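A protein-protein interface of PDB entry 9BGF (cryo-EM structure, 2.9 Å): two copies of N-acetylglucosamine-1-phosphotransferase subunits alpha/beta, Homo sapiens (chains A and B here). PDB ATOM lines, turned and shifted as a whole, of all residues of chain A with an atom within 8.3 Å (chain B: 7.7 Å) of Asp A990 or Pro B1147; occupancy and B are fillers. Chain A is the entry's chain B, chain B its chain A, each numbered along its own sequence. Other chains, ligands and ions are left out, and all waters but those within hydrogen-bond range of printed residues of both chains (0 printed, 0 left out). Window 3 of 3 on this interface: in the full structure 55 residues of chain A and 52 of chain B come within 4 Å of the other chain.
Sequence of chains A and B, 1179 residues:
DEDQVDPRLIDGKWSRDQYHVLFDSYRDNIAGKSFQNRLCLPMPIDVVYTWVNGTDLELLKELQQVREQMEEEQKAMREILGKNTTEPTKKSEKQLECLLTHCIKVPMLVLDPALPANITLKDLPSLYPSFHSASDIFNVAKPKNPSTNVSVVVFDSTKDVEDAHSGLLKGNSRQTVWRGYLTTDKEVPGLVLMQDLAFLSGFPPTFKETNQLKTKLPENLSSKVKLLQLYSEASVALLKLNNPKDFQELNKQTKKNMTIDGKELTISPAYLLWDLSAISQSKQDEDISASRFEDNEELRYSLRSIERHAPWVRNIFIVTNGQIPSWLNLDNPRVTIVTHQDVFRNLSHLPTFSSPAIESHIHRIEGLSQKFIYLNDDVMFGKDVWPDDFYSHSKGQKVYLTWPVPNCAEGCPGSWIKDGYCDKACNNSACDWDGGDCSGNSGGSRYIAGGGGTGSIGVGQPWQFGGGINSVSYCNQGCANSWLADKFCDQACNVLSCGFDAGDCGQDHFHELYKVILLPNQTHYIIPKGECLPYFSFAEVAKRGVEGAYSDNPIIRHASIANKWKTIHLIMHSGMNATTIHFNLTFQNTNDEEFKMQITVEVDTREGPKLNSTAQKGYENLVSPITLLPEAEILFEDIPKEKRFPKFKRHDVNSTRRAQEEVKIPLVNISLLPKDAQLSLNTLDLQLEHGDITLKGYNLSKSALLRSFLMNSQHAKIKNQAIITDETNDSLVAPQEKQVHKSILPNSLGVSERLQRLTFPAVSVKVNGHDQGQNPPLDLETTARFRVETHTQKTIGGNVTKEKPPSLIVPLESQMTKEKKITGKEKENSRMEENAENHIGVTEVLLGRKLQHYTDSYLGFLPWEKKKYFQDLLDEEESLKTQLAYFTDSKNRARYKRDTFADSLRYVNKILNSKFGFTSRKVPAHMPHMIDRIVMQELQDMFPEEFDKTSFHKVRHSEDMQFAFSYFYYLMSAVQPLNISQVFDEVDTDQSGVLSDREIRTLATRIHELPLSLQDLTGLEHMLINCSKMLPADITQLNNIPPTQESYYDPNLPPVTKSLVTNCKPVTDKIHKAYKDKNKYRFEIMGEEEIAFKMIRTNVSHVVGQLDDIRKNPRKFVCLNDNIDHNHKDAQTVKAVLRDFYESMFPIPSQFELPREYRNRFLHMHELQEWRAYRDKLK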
ATOM      1  N   PHE A 984     -34.182  33.654 -29.283  1.00  0.00           N
ATOM      2  CA  PHE A 984     -34.127  32.895 -28.041  1.00  0.00           C
ATOM      3  C   PHE A 984     -33.401  31.572 -28.237  1.00  0.00           C
ATOM      4  O   PHE A 984     -32.574  31.182 -27.405  1.00  0.00           O
ATOM      5  CB  PHE A 984     -35.536  32.658 -27.500  1.00  0.00           C
ATOM      6  CG  PHE A 984     -35.561  31.970 -26.168  1.00  0.00           C
ATOM      7  CD1 PHE A 984     -35.435  32.698 -24.999  1.00  0.00           C
ATOM      8  CD2 PHE A 984     -35.704  30.596 -26.084  1.00  0.00           C
ATOM      9  CE1 PHE A 984     -35.457  32.069 -23.776  1.00  0.00           C
ATOM     10  CE2 PHE A 984     -35.723  29.963 -24.861  1.00  0.00           C
ATOM     11  CZ  PHE A 984     -35.599  30.701 -23.707  1.00  0.00           C
ATOM     12  N   ASP A 985     -33.689  30.868 -29.335  1.00  0.00           N
ATOM     13  CA  ASP A 985     -33.043  29.581 -29.573  1.00  0.00           C
ATOM     14  C   ASP A 985     -31.541  29.736 -29.782  1.00  0.00           C
ATOM     15  O   ASP A 985     -30.759  28.883 -29.347  1.00  0.00           O
ATOM     16  CB  ASP A 985     -33.681  28.880 -30.769  1.00  0.00           C
ATOM     17  CG  ASP A 985     -34.964  28.164 -30.406  1.00  0.00           C
ATOM     18  OD1 ASP A 985     -35.499  28.426 -29.309  1.00  0.00           O
ATOM     19  OD2 ASP A 985     -35.432  27.332 -31.209  1.00  0.00           O
ATOM     20  N   GLU A 986     -31.118  30.805 -30.453  1.00  0.00           N
ATOM     21  CA  GLU A 986     -29.696  31.021 -30.674  1.00  0.00           C
ATOM     22  C   GLU A 986     -28.986  31.556 -29.439  1.00  0.00           C
ATOM     23  O   GLU A 986     -27.759  31.451 -29.356  1.00  0.00           O
ATOM     24  CB  GLU A 986     -29.481  31.967 -31.857  1.00  0.00           C
ATOM     25  CG  GLU A 986     -29.761  33.423 -31.561  1.00  0.00           C
ATOM     26  CD  GLU A 986     -29.717  34.281 -32.807  1.00  0.00           C
ATOM     27  OE1 GLU A 986     -30.024  33.758 -33.898  1.00  0.00           O
ATOM     28  OE2 GLU A 986     -29.374  35.477 -32.696  1.00  0.00           O
ATOM     29  N   VAL A 987     -29.718  32.124 -28.484  1.00  0.00           N
ATOM     30  CA  VAL A 987     -29.111  32.503 -27.211  1.00  0.00           C
ATOM     31  C   VAL A 987     -29.161  31.355 -26.209  1.00  0.00           C
ATOM     32  O   VAL A 987     -28.186  31.099 -25.501  1.00  0.00           O
ATOM     33  CB  VAL A 987     -29.784  33.773 -26.657  1.00  0.00           C
ATOM     34  CG1 VAL A 987     -29.368  34.008 -25.221  1.00  0.00           C
ATOM     35  CG2 VAL A 987     -29.415  34.971 -27.508  1.00  0.00           C
ATOM     36  N   ASP A 988     -30.283  30.644 -26.136  1.00  0.00           N
ATOM     37  CA  ASP A 988     -30.415  29.478 -25.264  1.00  0.00           C
ATOM     38  C   ASP A 988     -29.678  28.318 -25.920  1.00  0.00           C
ATOM     39  O   ASP A 988     -30.260  27.512 -26.644  1.00  0.00           O
ATOM     40  CB  ASP A 988     -31.883  29.152 -25.022  1.00  0.00           C
ATOM     41  CG  ASP A 988     -32.075  27.899 -24.198  1.00  0.00           C
ATOM     42  OD1 ASP A 988     -31.740  27.919 -22.997  1.00  0.00           O
ATOM     43  OD2 ASP A 988     -32.566  26.893 -24.750  1.00  0.00           O
ATOM     44  N   THR A 989     -28.373  28.229 -25.659  1.00  0.00           N
ATOM     45  CA  THR A 989     -27.519  27.273 -26.355  1.00  0.00           C
ATOM     46  C   THR A 989     -27.583  25.863 -25.783  1.00  0.00           C
ATOM     47  O   THR A 989     -27.104  24.931 -26.436  1.00  0.00           O
ATOM     48  CB  THR A 989     -26.066  27.752 -26.344  1.00  0.00           C
ATOM     49  OG1 THR A 989     -25.667  28.046 -25.001  1.00  0.00           O
ATOM     50  CG2 THR A 989     -25.908  28.999 -27.192  1.00  0.00           C
ATOM     51  N   ASP A 990     -28.153  25.676 -24.596  1.00  0.00           N
ATOM     52  CA  ASP A 990     -28.220  24.359 -23.978  1.00  0.00           C
ATOM     53  C   ASP A 990     -29.521  23.623 -24.272  1.00  0.00           C
ATOM     54  O   ASP A 990     -29.734  22.538 -23.721  1.00  0.00           O
ATOM     55  CB  ASP A 990     -28.028  24.478 -22.465  1.00  0.00           C
ATOM     56  CG  ASP A 990     -29.032  25.407 -21.830  1.00  0.00           C
ATOM     57  OD1 ASP A 990     -29.661  26.183 -22.574  1.00  0.00           O
ATOM     58  OD2 ASP A 990     -29.190  25.367 -20.592  1.00  0.00           O
ATOM     59  N   GLN A 991     -30.389  24.187 -25.115  1.00  0.00           N
ATOM     60  CA  GLN A 991     -31.654  23.556 -25.498  1.00  0.00           C
ATOM     61  C   GLN A 991     -32.510  23.231 -24.277  1.00  0.00           C
ATOM     62  O   GLN A 991     -33.131  22.169 -24.195  1.00  0.00           O
ATOM     63  CB  GLN A 991     -31.413  22.301 -26.343  1.00  0.00           C
ATOM     64  CG  GLN A 991     -31.297  22.558 -27.835  1.00  0.00           C
ATOM     65  CD  GLN A 991     -30.218  23.561 -28.177  1.00  0.00           C
ATOM     66  OE1 GLN A 991     -29.028  23.273 -28.061  1.00  0.00           O
ATOM     67  NE2 GLN A 991     -30.629  24.749 -28.604  1.00  0.00           N
ATOM     68  N   SER A 992     -32.538  24.150 -23.314  1.00  0.00           N
ATOM     69  CA  SER A 992     -33.304  23.957 -22.092  1.00  0.00           C
ATOM     70  C   SER A 992     -34.606  24.742 -22.071  1.00  0.00           C
ATOM     71  O   SER A 992     -35.516  24.381 -21.319  1.00  0.00           O
ATOM     72  CB  SER A 992     -32.465  24.353 -20.873  1.00  0.00           C
ATOM     73  OG  SER A 992     -32.095  25.720 -20.934  1.00  0.00           O
ATOM     74  N   GLY A 993     -34.714  25.793 -22.876  1.00  0.00           N
ATOM     75  CA  GLY A 993     -35.869  26.658 -22.852  1.00  0.00           C
ATOM     76  C   GLY A 993     -35.814  27.763 -21.822  1.00  0.00           C
ATOM     77  O   GLY A 993     -36.718  28.604 -21.796  1.00  0.00           O
ATOM     78  N   VAL A 994     -34.786  27.797 -20.979  1.00  0.00           N
ATOM     79  CA  VAL A 994     -34.642  28.814 -19.945  1.00  0.00           C
ATOM     80  C   VAL A 994     -33.260  29.434 -20.079  1.00  0.00           C
ATOM     81  O   VAL A 994     -32.268  28.719 -20.254  1.00  0.00           O
ATOM     82  CB  VAL A 994     -34.837  28.233 -18.530  1.00  0.00           C
ATOM     83  CG1 VAL A 994     -34.857  29.350 -17.500  1.00  0.00           C
ATOM     84  CG2 VAL A 994     -36.112  27.410 -18.452  1.00  0.00           C
ATOM     85  N   LEU A 995     -33.195  30.760 -20.005  1.00  0.00           N
ATOM     86  CA  LEU A 995     -31.925  31.466 -20.104  1.00  0.00           C
ATOM     87  C   LEU A 995     -31.226  31.464 -18.752  1.00  0.00           C
ATOM     88  O   LEU A 995     -31.770  31.966 -17.763  1.00  0.00           O
ATOM     89  CB  LEU A 995     -32.140  32.898 -20.587  1.00  0.00           C
ATOM     90  CG  LEU A 995     -32.623  33.090 -22.023  1.00  0.00           C
ATOM     91  CD1 LEU A 995     -32.551  34.554 -22.415  1.00  0.00           C
ATOM     92  CD2 LEU A 995     -31.823  32.235 -22.987  1.00  0.00           C
ATOM     93  N   SER A 996     -30.019  30.906 -18.710  1.00  0.00           N
ATOM     94  CA  SER A 996     -29.196  30.938 -17.514  1.00  0.00           C
ATOM     95  C   SER A 996     -28.482  32.285 -17.418  1.00  0.00           C
ATOM     96  O   SER A 996     -28.673  33.177 -18.247  1.00  0.00           O
ATOM     97  CB  SER A 996     -28.205  29.779 -17.527  1.00  0.00           C
ATOM     98  OG  SER A 996     -28.878  28.549 -17.724  1.00  0.00           O
ATOM     99  N   ARG A 998     -25.305  32.988 -17.866  1.00  0.00           N
ATOM    100  CA  ARG A 998     -24.418  33.189 -19.008  1.00  0.00           C
ATOM    101  C   ARG A 998     -25.203  33.518 -20.273  1.00  0.00           C
ATOM    102  O   ARG A 998     -24.798  34.383 -21.061  1.00  0.00           O
ATOM    103  CB  ARG A 998     -23.552  31.948 -19.211  1.00  0.00           C
ATOM    104  CG  ARG A 998     -24.317  30.642 -19.083  1.00  0.00           C
ATOM    105  CD  ARG A 998     -23.393  29.451 -19.230  1.00  0.00           C
ATOM    106  NE  ARG A 998     -22.366  29.424 -18.196  1.00  0.00           N
ATOM    107  CZ  ARG A 998     -22.330  28.550 -17.202  1.00  0.00           C
ATOM    108  NH1 ARG A 998     -23.248  27.605 -17.079  1.00  0.00           N
ATOM    109  NH2 ARG A 998     -21.347  28.621 -16.309  1.00  0.00           N
ATOM    110  N   GLU A 999     -26.327  32.832 -20.488  1.00  0.00           N
ATOM    111  CA  GLU A 999     -27.159  33.119 -21.649  1.00  0.00           C
ATOM    112  C   GLU A 999     -27.806  34.496 -21.542  1.00  0.00           C
ATOM    113  O   GLU A 999     -27.923  35.211 -22.541  1.00  0.00           O
ATOM    114  CB  GLU A 999     -28.202  32.018 -21.814  1.00  0.00           C
ATOM    115  CG  GLU A 999     -27.576  30.694 -22.201  1.00  0.00           C
ATOM    116  CD  GLU A 999     -28.422  29.499 -21.838  1.00  0.00           C
ATOM    117  OE1 GLU A 999     -29.533  29.685 -21.308  1.00  0.00           O
ATOM    118  OE2 GLU A 999     -27.970  28.363 -22.078  1.00  0.00           O
ATOM    119  N   GLU A1046     -31.970  25.066 -12.074  1.00  0.00           N
ATOM    120  CA  GLU A1046     -31.070  26.182 -12.335  1.00  0.00           C
ATOM    121  C   GLU A1046     -31.049  27.147 -11.157  1.00  0.00           C
ATOM    122  O   GLU A1046     -31.828  27.007 -10.216  1.00  0.00           O
ATOM    123  CB  GLU A1046     -31.483  26.919 -13.612  1.00  0.00           C
ATOM    124  CG  GLU A1046     -32.756  27.751 -13.486  1.00  0.00           C
ATOM    125  CD  GLU A1046     -34.028  26.926 -13.588  1.00  0.00           C
ATOM    126  OE1 GLU A1046     -34.093  25.829 -12.992  1.00  0.00           O
ATOM    127  OE2 GLU A1046     -34.969  27.377 -14.272  1.00  0.00           O
ATOM    128  N   TYR B 301     -13.855  22.267 -25.178  1.00  0.00           N
ATOM    129  CA  TYR B 301     -14.797  23.138 -25.860  1.00  0.00           C
ATOM    130  C   TYR B 301     -14.501  23.253 -27.346  1.00  0.00           C
ATOM    131  O   TYR B 301     -15.421  23.503 -28.124  1.00  0.00           O
ATOM    132  CB  TYR B 301     -14.796  24.509 -25.196  1.00  0.00           C
ATOM    133  CG  TYR B 301     -15.152  24.437 -23.730  1.00  0.00           C
ATOM    134  CD1 TYR B 301     -16.458  24.201 -23.327  1.00  0.00           C
ATOM    135  CD2 TYR B 301     -14.184  24.596 -22.750  1.00  0.00           C
ATOM    136  CE1 TYR B 301     -16.785  24.131 -21.990  1.00  0.00           C
ATOM    137  CE2 TYR B 301     -14.506  24.528 -21.413  1.00  0.00           C
ATOM    138  CZ  TYR B 301     -15.806  24.294 -21.039  1.00  0.00           C
ATOM    139  OH  TYR B 301     -16.134  24.226 -19.708  1.00  0.00           O
ATOM    140  N   ARG B 304     -16.228  20.257 -28.648  1.00  0.00           N
ATOM    141  CA  ARG B 304     -17.653  20.570 -28.668  1.00  0.00           C
ATOM    142  C   ARG B 304     -18.005  21.469 -29.849  1.00  0.00           C
ATOM    143  O   ARG B 304     -19.035  21.272 -30.505  1.00  0.00           O
ATOM    144  CB  ARG B 304     -18.065  21.227 -27.352  1.00  0.00           C
ATOM    145  CG  ARG B 304     -18.106  20.285 -26.165  1.00  0.00           C
ATOM    146  CD  ARG B 304     -18.384  21.052 -24.891  1.00  0.00           C
ATOM    147  NE  ARG B 304     -18.607  20.175 -23.750  1.00  0.00           N
ATOM    148  CZ  ARG B 304     -18.903  20.601 -22.531  1.00  0.00           C
ATOM    149  NH1 ARG B 304     -19.015  21.890 -22.258  1.00  0.00           N
ATOM    150  NH2 ARG B 304     -19.089  19.713 -21.559  1.00  0.00           N
ATOM    151  N   PHE B1141     -17.459  31.541 -20.320  1.00  0.00           N
ATOM    152  CA  PHE B1141     -17.684  31.907 -21.716  1.00  0.00           C
ATOM    153  C   PHE B1141     -17.819  30.667 -22.593  1.00  0.00           C
ATOM    154  O   PHE B1141     -18.729  30.568 -23.429  1.00  0.00           O
ATOM    155  CB  PHE B1141     -16.534  32.798 -22.183  1.00  0.00           C
ATOM    156  CG  PHE B1141     -16.552  33.109 -23.644  1.00  0.00           C
ATOM    157  CD1 PHE B1141     -17.443  34.033 -24.157  1.00  0.00           C
ATOM    158  CD2 PHE B1141     -15.652  32.505 -24.503  1.00  0.00           C
ATOM    159  CE1 PHE B1141     -17.449  34.330 -25.499  1.00  0.00           C
ATOM    160  CE2 PHE B1141     -15.655  32.801 -25.845  1.00  0.00           C
ATOM    161  CZ  PHE B1141     -16.554  33.715 -26.341  1.00  0.00           C
ATOM    162  N   TYR B1142     -16.928  29.696 -22.395  1.00  0.00           N
ATOM    163  CA  TYR B1142     -16.982  28.454 -23.155  1.00  0.00           C
ATOM    164  C   TYR B1142     -18.282  27.702 -22.904  1.00  0.00           C
ATOM    165  O   TYR B1142     -18.873  27.138 -23.831  1.00  0.00           O
ATOM    166  CB  TYR B1142     -15.786  27.579 -22.788  1.00  0.00           C
ATOM    167  CG  TYR B1142     -14.476  27.993 -23.419  1.00  0.00           C
ATOM    168  CD1 TYR B1142     -14.425  28.439 -24.728  1.00  0.00           C
ATOM    169  CD2 TYR B1142     -13.290  27.926 -22.702  1.00  0.00           C
ATOM    170  CE1 TYR B1142     -13.231  28.811 -25.306  1.00  0.00           C
ATOM    171  CE2 TYR B1142     -12.092  28.297 -23.271  1.00  0.00           C
ATOM    172  CZ  TYR B1142     -12.068  28.740 -24.574  1.00  0.00           C
ATOM    173  OH  TYR B1142     -10.876  29.113 -25.150  1.00  0.00           O
ATOM    174  N   GLU B1143     -18.729  27.661 -21.648  1.00  0.00           N
ATOM    175  CA  GLU B1143     -19.979  26.990 -21.312  1.00  0.00           C
ATOM    176  C   GLU B1143     -21.180  27.719 -21.892  1.00  0.00           C
ATOM    177  O   GLU B1143     -22.166  27.081 -22.270  1.00  0.00           O
ATOM    178  CB  GLU B1143     -20.113  26.864 -19.797  1.00  0.00           C
ATOM    179  CG  GLU B1143     -19.268  25.764 -19.187  1.00  0.00           C
ATOM    180  CD  GLU B1143     -19.882  24.391 -19.372  1.00  0.00           C
ATOM    181  OE1 GLU B1143     -21.068  24.314 -19.751  1.00  0.00           O
ATOM    182  OE2 GLU B1143     -19.178  23.389 -19.138  1.00  0.00           O
ATOM    183  N   SER B1144     -21.124  29.050 -21.961  1.00  0.00           N
ATOM    184  CA  SER B1144     -22.185  29.790 -22.631  1.00  0.00           C
ATOM    185  C   SER B1144     -22.245  29.434 -24.109  1.00  0.00           C
ATOM    186  O   SER B1144     -23.333  29.276 -24.673  1.00  0.00           O
ATOM    187  CB  SER B1144     -21.983  31.293 -22.450  1.00  0.00           C
ATOM    188  OG  SER B1144     -20.915  31.767 -23.247  1.00  0.00           O
ATOM    189  N   MET B1145     -21.084  29.306 -24.757  1.00  0.00           N
ATOM    190  CA  MET B1145     -21.086  28.940 -26.172  1.00  0.00           C
ATOM    191  C   MET B1145     -21.454  27.472 -26.378  1.00  0.00           C
ATOM    192  O   MET B1145     -22.283  27.149 -27.236  1.00  0.00           O
ATOM    193  CB  MET B1145     -19.729  29.252 -26.799  1.00  0.00           C
ATOM    194  CG  MET B1145     -19.420  30.732 -26.901  1.00  0.00           C
ATOM    195  SD  MET B1145     -17.933  31.065 -27.863  1.00  0.00           S
ATOM    196  CE  MET B1145     -18.504  30.719 -29.525  1.00  0.00           C
ATOM    197  N   PHE B1146     -20.852  26.564 -25.606  1.00  0.00           N
ATOM    198  CA  PHE B1146     -21.010  25.122 -25.811  1.00  0.00           C
ATOM    199  C   PHE B1146     -21.298  24.420 -24.491  1.00  0.00           C
ATOM    200  O   PHE B1146     -20.390  23.868 -23.856  1.00  0.00           O
ATOM    201  CB  PHE B1146     -19.771  24.530 -26.485  1.00  0.00           C
ATOM    202  CG  PHE B1146     -19.348  25.279 -27.710  1.00  0.00           C
ATOM    203  CD1 PHE B1146     -20.006  25.094 -28.912  1.00  0.00           C
ATOM    204  CD2 PHE B1146     -18.309  26.187 -27.654  1.00  0.00           C
ATOM    205  CE1 PHE B1146     -19.629  25.794 -30.035  1.00  0.00           C
ATOM    206  CE2 PHE B1146     -17.930  26.889 -28.775  1.00  0.00           C
ATOM    207  CZ  PHE B1146     -18.592  26.694 -29.964  1.00  0.00           C
ATOM    208  N   PRO B1147     -22.558  24.410 -24.052  1.00  0.00           N
ATOM    209  CA  PRO B1147     -22.890  23.750 -22.782  1.00  0.00           C
ATOM    210  C   PRO B1147     -22.997  22.237 -22.901  1.00  0.00           C
ATOM    211  O   PRO B1147     -22.653  21.513 -21.963  1.00  0.00           O
ATOM    212  CB  PRO B1147     -24.245  24.367 -22.406  1.00  0.00           C
ATOM    213  CG  PRO B1147     -24.516  25.442 -23.430  1.00  0.00           C
ATOM    214  CD  PRO B1147     -23.722  25.089 -24.633  1.00  0.00           C
ATOM    215  N   ILE B1148     -23.476  21.752 -24.042  1.00  0.00           N
ATOM    216  CA  ILE B1148     -23.785  20.334 -24.216  1.00  0.00           C
ATOM    217  C   ILE B1148     -22.500  19.531 -24.381  1.00  0.00           C
ATOM    218  O   ILE B1148     -21.694  19.834 -25.272  1.00  0.00           O
ATOM    219  CB  ILE B1148     -24.723  20.117 -25.413  1.00  0.00           C
ATOM    220  CG1 ILE B1148     -25.991  20.956 -25.253  1.00  0.00           C
ATOM    221  CG2 ILE B1148     -25.076  18.647 -25.551  1.00  0.00           C
ATOM    222  CD1 ILE B1148     -26.954  20.832 -26.411  1.00  0.00           C
ATOM    223  N   PRO B1149     -22.267  18.513 -23.554  1.00  0.00           N
ATOM    224  CA  PRO B1149     -21.059  17.694 -23.713  1.00  0.00           C
ATOM    225  C   PRO B1149     -21.047  16.974 -25.052  1.00  0.00           C
ATOM    226  O   PRO B1149     -22.084  16.548 -25.564  1.00  0.00           O
ATOM    227  CB  PRO B1149     -21.145  16.702 -22.548  1.00  0.00           C
ATOM    228  CG  PRO B1149     -22.072  17.337 -21.567  1.00  0.00           C
ATOM    229  CD  PRO B1149     -23.060  18.105 -22.384  1.00  0.00           C
ATOM    230  N   SER B1150     -19.849  16.833 -25.613  1.00  0.00           N
ATOM    231  CA  SER B1150     -19.694  16.211 -26.916  1.00  0.00           C
ATOM    232  C   SER B1150     -19.660  14.691 -26.790  1.00  0.00           C
ATOM    233  O   SER B1150     -19.671  14.125 -25.695  1.00  0.00           O
ATOM    234  CB  SER B1150     -18.426  16.712 -27.604  1.00  0.00           C
ATOM    235  OG  SER B1150     -17.271  16.368 -26.863  1.00  0.00           O
ATOM    236  N   GLU B1153     -16.442  12.874 -24.892  1.00  0.00           N
ATOM    237  CA  GLU B1153     -16.226  13.022 -23.463  1.00  0.00           C
ATOM    238  C   GLU B1153     -16.831  11.849 -22.710  1.00  0.00           C
ATOM    239  O   GLU B1153     -17.895  11.342 -23.078  1.00  0.00           O
ATOM    240  CB  GLU B1153     -16.838  14.317 -22.935  1.00  0.00           C
ATOM    241  CG  GLU B1153     -16.248  15.575 -23.512  1.00  0.00           C
ATOM    242  CD  GLU B1153     -16.631  16.790 -22.703  1.00  0.00           C
ATOM    243  OE1 GLU B1153     -16.351  16.805 -21.487  1.00  0.00           O
ATOM    244  OE2 GLU B1153     -17.221  17.727 -23.275  1.00  0.00           O
ATOM    245  N   ARG B1156     -19.401  12.681 -16.465  1.00  0.00           N
ATOM    246  CA  ARG B1156     -18.733  13.379 -15.371  1.00  0.00           C
ATOM    247  C   ARG B1156     -18.375  12.443 -14.223  1.00  0.00           C
ATOM    248  O   ARG B1156     -17.433  12.718 -13.471  1.00  0.00           O
ATOM    249  CB  ARG B1156     -19.615  14.520 -14.867  1.00  0.00           C
ATOM    250  CG  ARG B1156     -19.626  15.744 -15.765  1.00  0.00           C
ATOM    251  CD  ARG B1156     -18.303  16.486 -15.688  1.00  0.00           C
ATOM    252  NE  ARG B1156     -18.313  17.721 -16.461  1.00  0.00           N
ATOM    253  CZ  ARG B1156     -17.325  18.606 -16.468  1.00  0.00           C
ATOM    254  NH1 ARG B1156     -16.231  18.425 -15.746  1.00  0.00           N
ATOM    255  NH2 ARG B1156     -17.438  19.699 -17.217  1.00  0.00           N
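Among the printed residues, merely in contact across the chains: Thr A989 with Met B1145 (3.9 Å), Thr A989 with Pro B1147 (3.3 Å), Asp A990 with Pro B1147 (3.8 Å), Gln A991 with Ile B1148 (3.6 Å), Arg A998 with Glu B1143 (3.8 Å) and Arg A998 with Ser B1144 (3.6 Å).
No position is printed for both chains.
Of the 7 pairs that touch across the chains among the printed residues, none has its exchanged pair printed and touching as well.
Of chain B, only Pro B1147 (3.8 Å) comes within 4 Å of Asp A990.
Pro B1147 touches two residues of chain A.
Of the printed residues of chain A, Met B1145 touches Thr A989.
Of the printed residues of chain B, Arg A998 touches Glu B1143 and Ser B1144.
Phe B1146 touches none of the printed residues of chain A.
The nearest printed residue of chain A that does not touch Glu B1143 is Thr A989 (4.5 Å).
OH of Tyr B301 lies within hydrogen-bond range of OE2 of Glu B1143 (3.2 Å).
OE2 of Glu B1143 is in salt-bridge range of NH1 of Arg B304, 3.5 Å away.
The guanidinium group of Arg B304 lies within hydrogen-bond range of the backbone carbonyl oxygen of Ile B1148, at 3.5 Å.
The backbone carbonyl oxygen of Phe B1141 sits at hydrogen-bond distance from the side-chain hydroxyl of Ser B1144 (2.5 Å).
O of Asp A988 lies within hydrogen-bond range of NE2 of Gln A991, at 3.4 Å.
The side-chain amide oxygen of Gln A991 sits close to the backbone carbonyl oxygen of Thr A989, 3.0 Å away.
The backbone carbonyl oxygen (O) of Ser B1144 sits at hydrogen-bond distance from the side-chain hydroxyl (OG1) of Thr A989 (2.7 Å).
Printed residues of chain B that touch a printed residue of chain A: Glu B1143, Ser B1144, Met B1145, Pro B1147 and Ile B1148.
Among the printed residues, 7 pairs touch across the chains.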
